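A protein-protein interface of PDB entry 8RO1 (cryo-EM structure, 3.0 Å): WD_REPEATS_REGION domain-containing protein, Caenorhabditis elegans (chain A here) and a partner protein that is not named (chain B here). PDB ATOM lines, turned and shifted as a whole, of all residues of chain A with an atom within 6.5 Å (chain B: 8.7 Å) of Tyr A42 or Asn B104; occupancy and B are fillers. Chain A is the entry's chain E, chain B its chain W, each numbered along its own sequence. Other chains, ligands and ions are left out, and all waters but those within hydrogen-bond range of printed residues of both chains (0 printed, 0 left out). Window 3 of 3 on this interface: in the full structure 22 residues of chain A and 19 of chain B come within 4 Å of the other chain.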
ATOM      1  N   GLY A  39       0.910  -9.280  22.291  1.00  0.00           N
ATOM      2  CA  GLY A  39       1.615  -8.382  23.171  1.00  0.00           C
ATOM      3  C   GLY A  39       3.107  -8.676  23.214  1.00  0.00           C
ATOM      4  O   GLY A  39       3.571  -9.751  22.843  1.00  0.00           O
ATOM      5  N   GLU A  40       3.859  -7.688  23.673  1.00  0.00           N
ATOM      6  CA  GLU A  40       5.288  -7.842  23.925  1.00  0.00           C
ATOM      7  C   GLU A  40       5.558  -8.755  25.116  1.00  0.00           C
ATOM      8  O   GLU A  40       5.128  -8.462  26.232  1.00  0.00           O
ATOM      9  CB  GLU A  40       5.942  -6.489  24.181  1.00  0.00           C
ATOM     10  CG  GLU A  40       5.803  -5.454  23.089  1.00  0.00           C
ATOM     11  CD  GLU A  40       6.147  -4.070  23.591  1.00  0.00           C
ATOM     12  OE1 GLU A  40       6.880  -3.979  24.599  1.00  0.00           O
ATOM     13  OE2 GLU A  40       5.689  -3.079  22.987  1.00  0.00           O
ATOM     14  N   ILE A  41       6.228  -9.878  24.882  1.00  0.00           N
ATOM     15  CA  ILE A  41       6.321 -10.941  25.876  1.00  0.00           C
ATOM     16  C   ILE A  41       7.448 -10.555  26.824  1.00  0.00           C
ATOM     17  O   ILE A  41       8.612 -10.476  26.422  1.00  0.00           O
ATOM     18  CB  ILE A  41       6.591 -12.304  25.226  1.00  0.00           C
ATOM     19  CG1 ILE A  41       5.667 -12.547  24.020  1.00  0.00           C
ATOM     20  CG2 ILE A  41       6.422 -13.429  26.251  1.00  0.00           C
ATOM     21  CD1 ILE A  41       5.979 -13.770  23.262  1.00  0.00           C
ATOM     22  N   TYR A  42       7.100 -10.341  28.092  1.00  0.00           N
ATOM     23  CA  TYR A  42       7.993  -9.857  29.137  1.00  0.00           C
ATOM     24  C   TYR A  42       8.479 -10.924  30.100  1.00  0.00           C
ATOM     25  O   TYR A  42       9.309 -10.614  30.953  1.00  0.00           O
ATOM     26  CB  TYR A  42       7.285  -8.761  29.944  1.00  0.00           C
ATOM     27  CG  TYR A  42       7.103  -7.421  29.261  1.00  0.00           C
ATOM     28  CD1 TYR A  42       7.313  -7.249  27.899  1.00  0.00           C
ATOM     29  CD2 TYR A  42       6.664  -6.336  29.975  1.00  0.00           C
ATOM     30  CE1 TYR A  42       7.169  -6.034  27.309  1.00  0.00           C
ATOM     31  CE2 TYR A  42       6.477  -5.129  29.372  1.00  0.00           C
ATOM     32  CZ  TYR A  42       6.723  -4.988  28.037  1.00  0.00           C
ATOM     33  OH  TYR A  42       6.510  -3.783  27.416  1.00  0.00           O
ATOM     34  N   THR A  43       7.972 -12.147  30.022  1.00  0.00           N
ATOM     35  CA  THR A  43       8.377 -13.177  30.968  1.00  0.00           C
ATOM     36  C   THR A  43       8.000 -14.553  30.456  1.00  0.00           C
ATOM     37  O   THR A  43       7.025 -14.712  29.724  1.00  0.00           O
ATOM     38  CB  THR A  43       7.761 -12.918  32.345  1.00  0.00           C
ATOM     39  OG1 THR A  43       8.257 -13.880  33.277  1.00  0.00           O
ATOM     40  CG2 THR A  43       6.234 -12.906  32.323  1.00  0.00           C
ATOM     41  N   GLY A  44       8.776 -15.543  30.865  1.00  0.00           N
ATOM     42  CA  GLY A  44       8.488 -16.914  30.512  1.00  0.00           C
ATOM     43  C   GLY A  44       9.310 -17.889  31.319  1.00  0.00           C
ATOM     44  O   GLY A  44      10.495 -17.663  31.567  1.00  0.00           O
ATOM     45  N   SER A  56       4.112 -14.672  29.299  1.00  0.00           N
ATOM     46  CA  SER A  56       3.156 -13.580  29.319  1.00  0.00           C
ATOM     47  C   SER A  56       3.898 -12.264  29.236  1.00  0.00           C
ATOM     48  O   SER A  56       5.112 -12.193  29.413  1.00  0.00           O
ATOM     49  CB  SER A  56       2.286 -13.614  30.569  1.00  0.00           C
ATOM     50  OG  SER A  56       1.164 -12.773  30.393  1.00  0.00           O
ATOM     51  N   GLY A  57       3.132 -11.214  29.006  1.00  0.00           N
ATOM     52  CA  GLY A  57       3.644  -9.869  28.967  1.00  0.00           C
ATOM     53  C   GLY A  57       2.508  -8.917  28.699  1.00  0.00           C
ATOM     54  O   GLY A  57       1.429  -9.037  29.278  1.00  0.00           O
ATOM     55  N   TYR A  58       2.762  -7.949  27.821  1.00  0.00           N
ATOM     56  CA  TYR A  58       1.845  -6.834  27.628  1.00  0.00           C
ATOM     57  C   TYR A  58       0.464  -7.262  27.156  1.00  0.00           C
ATOM     58  O   TYR A  58      -0.498  -6.508  27.326  1.00  0.00           O
ATOM     59  CB  TYR A  58       2.453  -5.910  26.580  1.00  0.00           C
ATOM     60  CG  TYR A  58       1.996  -4.499  26.594  1.00  0.00           C
ATOM     61  CD1 TYR A  58       2.560  -3.580  27.445  1.00  0.00           C
ATOM     62  CD2 TYR A  58       1.024  -4.069  25.724  1.00  0.00           C
ATOM     63  CE1 TYR A  58       2.145  -2.283  27.448  1.00  0.00           C
ATOM     64  CE2 TYR A  58       0.609  -2.777  25.718  1.00  0.00           C
ATOM     65  CZ  TYR A  58       1.179  -1.882  26.576  1.00  0.00           C
ATOM     66  OH  TYR A  58       0.764  -0.570  26.566  1.00  0.00           O
ATOM     67  N   ALA A  83      -0.321  -5.379  32.557  1.00  0.00           N
ATOM     68  CA  ALA A  83       0.646  -6.251  31.895  1.00  0.00           C
ATOM     69  C   ALA A  83       1.465  -6.998  32.934  1.00  0.00           C
ATOM     70  O   ALA A  83       1.684  -6.498  34.039  1.00  0.00           O
ATOM     71  CB  ALA A  83       1.589  -5.427  31.028  1.00  0.00           C
ATOM     72  N   VAL A  84       1.956  -8.184  32.575  1.00  0.00           N
ATOM     73  CA  VAL A  84       2.540  -9.089  33.555  1.00  0.00           C
ATOM     74  C   VAL A  84       4.053  -9.017  33.458  1.00  0.00           C
ATOM     75  O   VAL A  84       4.653  -9.372  32.439  1.00  0.00           O
ATOM     76  CB  VAL A  84       2.054 -10.528  33.286  1.00  0.00           C
ATOM     77  CG1 VAL A  84       2.577 -11.529  34.297  1.00  0.00           C
ATOM     78  CG2 VAL A  84       0.536 -10.603  33.218  1.00  0.00           C
ATOM     79  N   MET A  85       4.642  -8.588  34.572  1.00  0.00           N
ATOM     80  CA  MET A  85       6.072  -8.325  34.704  1.00  0.00           C
ATOM     81  C   MET A  85       6.895  -9.596  34.761  1.00  0.00           C
ATOM     82  O   MET A  85       7.957  -9.681  34.138  1.00  0.00           O
ATOM     83  CB  MET A  85       6.349  -7.424  35.897  1.00  0.00           C
ATOM     84  CG  MET A  85       5.530  -6.140  35.893  1.00  0.00           C
ATOM     85  SD  MET A  85       5.755  -5.122  34.416  1.00  0.00           S
ATOM     86  CE  MET A  85       7.374  -4.415  34.691  1.00  0.00           C
ATOM     87  N   ASP A  86       6.432 -10.588  35.510  1.00  0.00           N
ATOM     88  CA  ASP A  86       7.225 -11.758  35.840  1.00  0.00           C
ATOM     89  C   ASP A  86       6.304 -12.827  36.370  1.00  0.00           C
ATOM     90  O   ASP A  86       5.260 -12.546  36.953  1.00  0.00           O
ATOM     91  CB  ASP A  86       8.288 -11.426  36.895  1.00  0.00           C
ATOM     92  CG  ASP A  86       9.374 -12.480  36.996  1.00  0.00           C
ATOM     93  OD1 ASP A  86       9.384 -13.431  36.190  1.00  0.00           O
ATOM     94  OD2 ASP A  86      10.222 -12.358  37.905  1.00  0.00           O
ATOM     95  N   PHE A 256      17.491   1.532  25.011  1.00  0.00           N
ATOM     96  CA  PHE A 256      16.685   2.637  25.522  1.00  0.00           C
ATOM     97  C   PHE A 256      15.300   2.234  26.006  1.00  0.00           C
ATOM     98  O   PHE A 256      14.673   3.010  26.730  1.00  0.00           O
ATOM     99  CB  PHE A 256      16.466   3.690  24.422  1.00  0.00           C
ATOM    100  CG  PHE A 256      15.924   3.132  23.111  1.00  0.00           C
ATOM    101  CD1 PHE A 256      14.581   2.876  22.944  1.00  0.00           C
ATOM    102  CD2 PHE A 256      16.765   2.819  22.078  1.00  0.00           C
ATOM    103  CE1 PHE A 256      14.096   2.321  21.795  1.00  0.00           C
ATOM    104  CE2 PHE A 256      16.275   2.271  20.913  1.00  0.00           C
ATOM    105  CZ  PHE A 256      14.942   2.018  20.779  1.00  0.00           C
ATOM    106  N   GLU A 257      14.799   1.047  25.649  1.00  0.00           N
ATOM    107  CA  GLU A 257      13.557   0.565  26.258  1.00  0.00           C
ATOM    108  C   GLU A 257      13.619   0.383  27.762  1.00  0.00           C
ATOM    109  O   GLU A 257      12.562   0.296  28.385  1.00  0.00           O
ATOM    110  CB  GLU A 257      13.073  -0.726  25.613  1.00  0.00           C
ATOM    111  CG  GLU A 257      13.062  -0.684  24.112  1.00  0.00           C
ATOM    112  CD  GLU A 257      12.436  -1.905  23.528  1.00  0.00           C
ATOM    113  OE1 GLU A 257      12.326  -2.919  24.242  1.00  0.00           O
ATOM    114  OE2 GLU A 257      12.030  -1.844  22.358  1.00  0.00           O
ATOM    115  N   ASN A 259      14.035  -2.133  29.573  1.00  0.00           N
ATOM    116  CA  ASN A 259      13.233  -3.256  30.043  1.00  0.00           C
ATOM    117  C   ASN A 259      13.880  -3.858  31.285  1.00  0.00           C
ATOM    118  O   ASN A 259      15.076  -3.717  31.522  1.00  0.00           O
ATOM    119  CB  ASN A 259      13.056  -4.343  28.986  1.00  0.00           C
ATOM    120  CG  ASN A 259      12.259  -3.883  27.806  1.00  0.00           C
ATOM    121  OD1 ASN A 259      11.631  -2.835  27.848  1.00  0.00           O
ATOM    122  ND2 ASN A 259      12.223  -4.699  26.763  1.00  0.00           N
ATOM    123  N   LEU A 260      13.059  -4.534  32.085  1.00  0.00           N
ATOM    124  CA  LEU A 260      13.544  -5.415  33.145  1.00  0.00           C
ATOM    125  C   LEU A 260      13.906  -6.803  32.612  1.00  0.00           C
ATOM    126  O   LEU A 260      13.298  -7.808  32.967  1.00  0.00           O
ATOM    127  CB  LEU A 260      12.510  -5.517  34.254  1.00  0.00           C
ATOM    128  CG  LEU A 260      11.936  -4.232  34.839  1.00  0.00           C
ATOM    129  CD1 LEU A 260      11.004  -4.603  35.940  1.00  0.00           C
ATOM    130  CD2 LEU A 260      12.998  -3.298  35.365  1.00  0.00           C
ATOM    131  N   LYS A 262      15.333 -10.196  32.366  1.00  0.00           N
ATOM    132  CA  LYS A 262      15.481 -11.208  33.403  1.00  0.00           C
ATOM    133  C   LYS A 262      16.817 -11.938  33.279  1.00  0.00           C
ATOM    134  O   LYS A 262      17.649 -11.624  32.429  1.00  0.00           O
ATOM    135  CB  LYS A 262      14.325 -12.203  33.326  1.00  0.00           C
ATOM    136  CG  LYS A 262      12.910 -11.606  33.310  1.00  0.00           C
ATOM    137  CD  LYS A 262      12.614 -10.719  34.506  1.00  0.00           C
ATOM    138  CE  LYS A 262      11.212 -10.159  34.444  1.00  0.00           C
ATOM    139  NZ  LYS A 262      10.963  -9.098  35.456  1.00  0.00           N
ATOM    140  N   ASN A 303      13.434 -10.331  26.360  1.00  0.00           N
ATOM    141  CA  ASN A 303      13.170  -9.912  27.726  1.00  0.00           C
ATOM    142  C   ASN A 303      13.483 -10.993  28.749  1.00  0.00           C
ATOM    143  O   ASN A 303      13.914 -10.669  29.857  1.00  0.00           O
ATOM    144  CB  ASN A 303      11.711  -9.496  27.842  1.00  0.00           C
ATOM    145  CG  ASN A 303      11.384  -8.312  26.975  1.00  0.00           C
ATOM    146  OD1 ASN A 303      12.102  -7.318  26.978  1.00  0.00           O
ATOM    147  ND2 ASN A 303      10.319  -8.420  26.195  1.00  0.00           N
ATOM    148  N   CYS A 304      13.293 -12.263  28.407  1.00  0.00           N
ATOM    149  CA  CYS A 304      13.425 -13.357  29.362  1.00  0.00           C
ATOM    150  C   CYS A 304      14.093 -14.558  28.720  1.00  0.00           C
ATOM    151  O   CYS A 304      13.956 -14.789  27.520  1.00  0.00           O
ATOM    152  CB  CYS A 304      12.068 -13.759  29.925  1.00  0.00           C
ATOM    153  SG  CYS A 304      12.143 -14.917  31.292  1.00  0.00           S
ATOM    154  N   CYS A 317      11.989 -15.436  25.427  1.00  0.00           N
ATOM    155  CA  CYS A 317      10.814 -14.625  25.160  1.00  0.00           C
ATOM    156  C   CYS A 317      11.270 -13.216  24.857  1.00  0.00           C
ATOM    157  O   CYS A 317      12.139 -12.689  25.556  1.00  0.00           O
ATOM    158  CB  CYS A 317       9.855 -14.623  26.339  1.00  0.00           C
ATOM    159  SG  CYS A 317       9.194 -16.240  26.742  1.00  0.00           S
ATOM    160  N   GLY A 318      10.698 -12.614  23.817  1.00  0.00           N
ATOM    161  CA  GLY A 318      11.197 -11.365  23.291  1.00  0.00           C
ATOM    162  C   GLY A 318      10.082 -10.360  23.082  1.00  0.00           C
ATOM    163  O   GLY A 318       8.903 -10.696  23.066  1.00  0.00           O
ATOM    164  N   SER A 319      10.496  -9.107  22.892  1.00  0.00           N
ATOM    165  CA  SER A 319       9.588  -8.043  22.482  1.00  0.00           C
ATOM    166  C   SER A 319       9.060  -8.228  21.065  1.00  0.00           C
ATOM    167  O   SER A 319       8.173  -7.473  20.663  1.00  0.00           O
ATOM    168  CB  SER A 319      10.272  -6.688  22.592  1.00  0.00           C
ATOM    169  OG  SER A 319       9.340  -5.644  22.393  1.00  0.00           O
ATOM    170  N   ALA B 101      12.029  -5.310  12.850  1.00  0.00           N
ATOM    171  CA  ALA B 101      12.269  -5.003  14.240  1.00  0.00           C
ATOM    172  C   ALA B 101      10.945  -4.725  14.920  1.00  0.00           C
ATOM    173  O   ALA B 101       9.954  -4.368  14.283  1.00  0.00           O
ATOM    174  CB  ALA B 101      13.216  -3.822  14.406  1.00  0.00           C
ATOM    175  N   HIS B 102      10.945  -4.907  16.229  1.00  0.00           N
ATOM    176  CA  HIS B 102       9.827  -4.564  17.088  1.00  0.00           C
ATOM    177  C   HIS B 102      10.368  -3.819  18.285  1.00  0.00           C
ATOM    178  O   HIS B 102      11.414  -4.192  18.817  1.00  0.00           O
ATOM    179  CB  HIS B 102       9.091  -5.783  17.609  1.00  0.00           C
ATOM    180  CG  HIS B 102       8.536  -6.685  16.555  1.00  0.00           C
ATOM    181  ND1 HIS B 102       9.289  -7.659  15.940  1.00  0.00           N
ATOM    182  CD2 HIS B 102       7.284  -6.815  16.064  1.00  0.00           C
ATOM    183  CE1 HIS B 102       8.533  -8.325  15.088  1.00  0.00           C
ATOM    184  NE2 HIS B 102       7.312  -7.830  15.142  1.00  0.00           N
ATOM    185  N   LEU B 103       9.656  -2.774  18.715  1.00  0.00           N
ATOM    186  CA  LEU B 103      10.092  -2.056  19.893  1.00  0.00           C
ATOM    187  C   LEU B 103       8.896  -1.629  20.728  1.00  0.00           C
ATOM    188  O   LEU B 103       7.738  -1.823  20.350  1.00  0.00           O
ATOM    189  CB  LEU B 103      10.858  -0.808  19.464  1.00  0.00           C
ATOM    190  CG  LEU B 103      12.195  -0.924  18.763  1.00  0.00           C
ATOM    191  CD1 LEU B 103      12.594   0.479  18.389  1.00  0.00           C
ATOM    192  CD2 LEU B 103      13.242  -1.559  19.630  1.00  0.00           C
ATOM    193  N   ASN B 104       9.204  -1.055  21.885  1.00  0.00           N
ATOM    194  CA  ASN B 104       8.244  -0.546  22.850  1.00  0.00           C
ATOM    195  C   ASN B 104       7.460   0.712  22.481  1.00  0.00           C
ATOM    196  O   ASN B 104       7.331   1.585  23.343  1.00  0.00           O
ATOM    197  CB  ASN B 104       8.953  -0.391  24.197  1.00  0.00           C
ATOM    198  CG  ASN B 104       7.986  -0.314  25.360  1.00  0.00           C
ATOM    199  OD1 ASN B 104       7.893   0.710  26.027  1.00  0.00           O
ATOM    200  ND2 ASN B 104       7.198  -1.360  25.546  1.00  0.00           N
ATOM    201  N   GLU B 105       6.917   0.825  21.260  1.00  0.00           N
ATOM    202  CA  GLU B 105       6.502   2.049  20.547  1.00  0.00           C
ATOM    203  C   GLU B 105       6.686   3.368  21.303  1.00  0.00           C
ATOM    204  O   GLU B 105       7.293   4.316  20.805  1.00  0.00           O
ATOM    205  CB  GLU B 105       5.028   1.854  20.148  1.00  0.00           C
ATOM    206  CG  GLU B 105       4.224   3.031  19.550  1.00  0.00           C
ATOM    207  CD  GLU B 105       4.372   3.152  18.044  1.00  0.00           C
ATOM    208  OE1 GLU B 105       4.114   2.154  17.337  1.00  0.00           O
ATOM    209  OE2 GLU B 105       4.735   4.245  17.560  1.00  0.00           O
ATOM    210  N   PHE B 106       6.104   3.417  22.500  1.00  0.00           N
ATOM    211  CA  PHE B 106       6.169   4.564  23.401  1.00  0.00           C
ATOM    212  C   PHE B 106       7.589   5.046  23.660  1.00  0.00           C
ATOM    213  O   PHE B 106       7.870   6.245  23.598  1.00  0.00           O
ATOM    214  CB  PHE B 106       5.539   4.204  24.744  1.00  0.00           C
ATOM    215  CG  PHE B 106       5.939   5.127  25.871  1.00  0.00           C
ATOM    216  CD1 PHE B 106       5.673   6.479  25.823  1.00  0.00           C
ATOM    217  CD2 PHE B 106       6.570   4.632  26.980  1.00  0.00           C
ATOM    218  CE1 PHE B 106       6.032   7.302  26.853  1.00  0.00           C
ATOM    219  CE2 PHE B 106       6.931   5.450  28.008  1.00  0.00           C
ATOM    220  CZ  PHE B 106       6.660   6.790  27.947  1.00  0.00           C
ATOM    221  N   HIS B 107       8.496   4.131  23.955  1.00  0.00           N
ATOM    222  CA  HIS B 107       9.891   4.518  24.115  1.00  0.00           C
ATOM    223  C   HIS B 107      10.537   4.910  22.801  1.00  0.00           C
ATOM    224  O   HIS B 107      11.328   5.852  22.773  1.00  0.00           O
ATOM    225  CB  HIS B 107      10.661   3.367  24.758  1.00  0.00           C
ATOM    226  CG  HIS B 107      10.689   3.409  26.253  1.00  0.00           C
ATOM    227  ND1 HIS B 107      10.545   2.276  27.019  1.00  0.00           N
ATOM    228  CD2 HIS B 107      10.978   4.410  27.117  1.00  0.00           C
ATOM    229  CE1 HIS B 107      10.660   2.592  28.295  1.00  0.00           C
ATOM    230  NE2 HIS B 107      10.941   3.877  28.381  1.00  0.00           N
ATOM    231  N   PHE B 108      10.256   4.207  21.710  1.00  0.00           N
ATOM    232  CA  PHE B 108      10.768   4.670  20.421  1.00  0.00           C
ATOM    233  C   PHE B 108      10.272   6.078  20.105  1.00  0.00           C
ATOM    234  O   PHE B 108      11.023   6.908  19.592  1.00  0.00           O
ATOM    235  CB  PHE B 108      10.366   3.709  19.307  1.00  0.00           C
ATOM    236  CG  PHE B 108      10.322   4.347  17.952  1.00  0.00           C
ATOM    237  CD1 PHE B 108      11.491   4.604  17.301  1.00  0.00           C
ATOM    238  CD2 PHE B 108       9.146   4.765  17.375  1.00  0.00           C
ATOM    239  CE1 PHE B 108      11.503   5.195  16.098  1.00  0.00           C
ATOM    240  CE2 PHE B 108       9.165   5.390  16.164  1.00  0.00           C
ATOM    241  CZ  PHE B 108      10.342   5.575  15.520  1.00  0.00           C
ATOM    242  N   ASN B 109       9.008   6.362  20.416  1.00  0.00           N
ATOM    243  CA  ASN B 109       8.457   7.709  20.263  1.00  0.00           C
ATOM    244  C   ASN B 109       9.195   8.725  21.100  1.00  0.00           C
ATOM    245  O   ASN B 109       9.416   9.855  20.665  1.00  0.00           O
ATOM    246  CB  ASN B 109       6.982   7.752  20.621  1.00  0.00           C
ATOM    247  CG  ASN B 109       6.116   7.370  19.471  1.00  0.00           C
ATOM    248  OD1 ASN B 109       5.942   8.147  18.539  1.00  0.00           O
ATOM    249  ND2 ASN B 109       5.545   6.192  19.526  1.00  0.00           N
ATOM    250  N   ARG B 110       9.575   8.343  22.307  1.00  0.00           N
ATOM    251  CA  ARG B 110      10.336   9.232  23.163  1.00  0.00           C
ATOM    252  C   ARG B 110      11.671   9.592  22.527  1.00  0.00           C
ATOM    253  O   ARG B 110      12.092  10.749  22.568  1.00  0.00           O
ATOM    254  CB  ARG B 110      10.538   8.551  24.510  1.00  0.00           C
ATOM    255  CG  ARG B 110      11.228   9.388  25.531  1.00  0.00           C
ATOM    256  CD  ARG B 110      11.208   8.745  26.909  1.00  0.00           C
ATOM    257  NE  ARG B 110      12.346   9.208  27.701  1.00  0.00           N
ATOM    258  CZ  ARG B 110      12.324  10.083  28.703  1.00  0.00           C
ATOM    259  NH1 ARG B 110      13.473  10.435  29.271  1.00  0.00           N
ATOM    260  NH2 ARG B 110      11.199  10.613  29.161  1.00  0.00           N
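OE2 of Glu A257 sits at hydrogen-bond distance from N of Asn B104, 3.0 Å away.
The backbone carbonyl oxygen of Glu A257 lies close to a ring nitrogen (ND1) of His B107 (3.1 Å).
ND2 of Asn B104 lies within hydrogen-bond range of OH of Tyr A42, 3.1 Å away.
The side-chain carboxylate of Glu A40 lies within hydrogen-bond range of the side-chain amide nitrogen of Asn B104 (2.8 Å).
The side-chain amide nitrogen (ND2) of Asn A259 sits at hydrogen-bond distance from the side-chain carboxylate (OE1) of Glu A257, at 3.1 Å.
O of Ser A56 is in hydrogen-bond range of N of Tyr A42 (3.0 Å).
OD1 of Asn B104 is in hydrogen-bond range of ND1 of His B107.
The backbone carbonyl oxygen of Glu A40 lies within hydrogen-bond range of the backbone NH of Tyr A58 (2.9 Å).
ND2 of Asn A303 sits close to N of Ser A319 (3.4 Å).
OH of Tyr A42 is in hydrogen-bond range of OE1 of Glu A40 (2.8 Å).
Glu A40 touches Leu B103 (OE2 to O, 3.6 Å).
Phe A256 touches Leu B103 (CZ to CD1, 3.7 Å).
O of Phe A256 touches CD2 of His B107, 3.97 Å away.
Glu A257 touches Leu B103 (OE2 to CD2, 3.0 Å).
Ser A319 touches His B102.
Tyr A42 touches one residue of chain B.
No residue of chain B comes within 4 Å of Thr A43.
Of the printed residues of chain B, Glu A257 touches Leu B103 (3.0 Å), Asn B104 (3.0 Å) and His B107 (3.0 Å).
Of the printed residues of chain A, His B102 touches Ser A319.
Printed residues of chain A within 4 Å of Leu B103: Glu A40 (3.6 Å), Phe A256 (3.7 Å) and Glu A257 (3.0 Å).
Asn B104 touches three residues of chain A.
The nearest residue of chain A that does not touch Asn B104 is Ser A319 (4.6 Å).
The nearest printed residue of chain B that does not touch Glu A40 is Glu B105 (4.4 Å).
Hydrophobic or aromatic side chains of chain A within 4 Å of the printed part of chain B: Tyr A42 and Phe A256.
Hydrophobic or aromatic side chains of chain B that line the printed part of chain A: His B102, Leu B103 and His B107.
Among the printed residues, no Asp or Glu carboxylate lies within 4 Å of a Lys or Arg side-chain nitrogen of the other chain.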
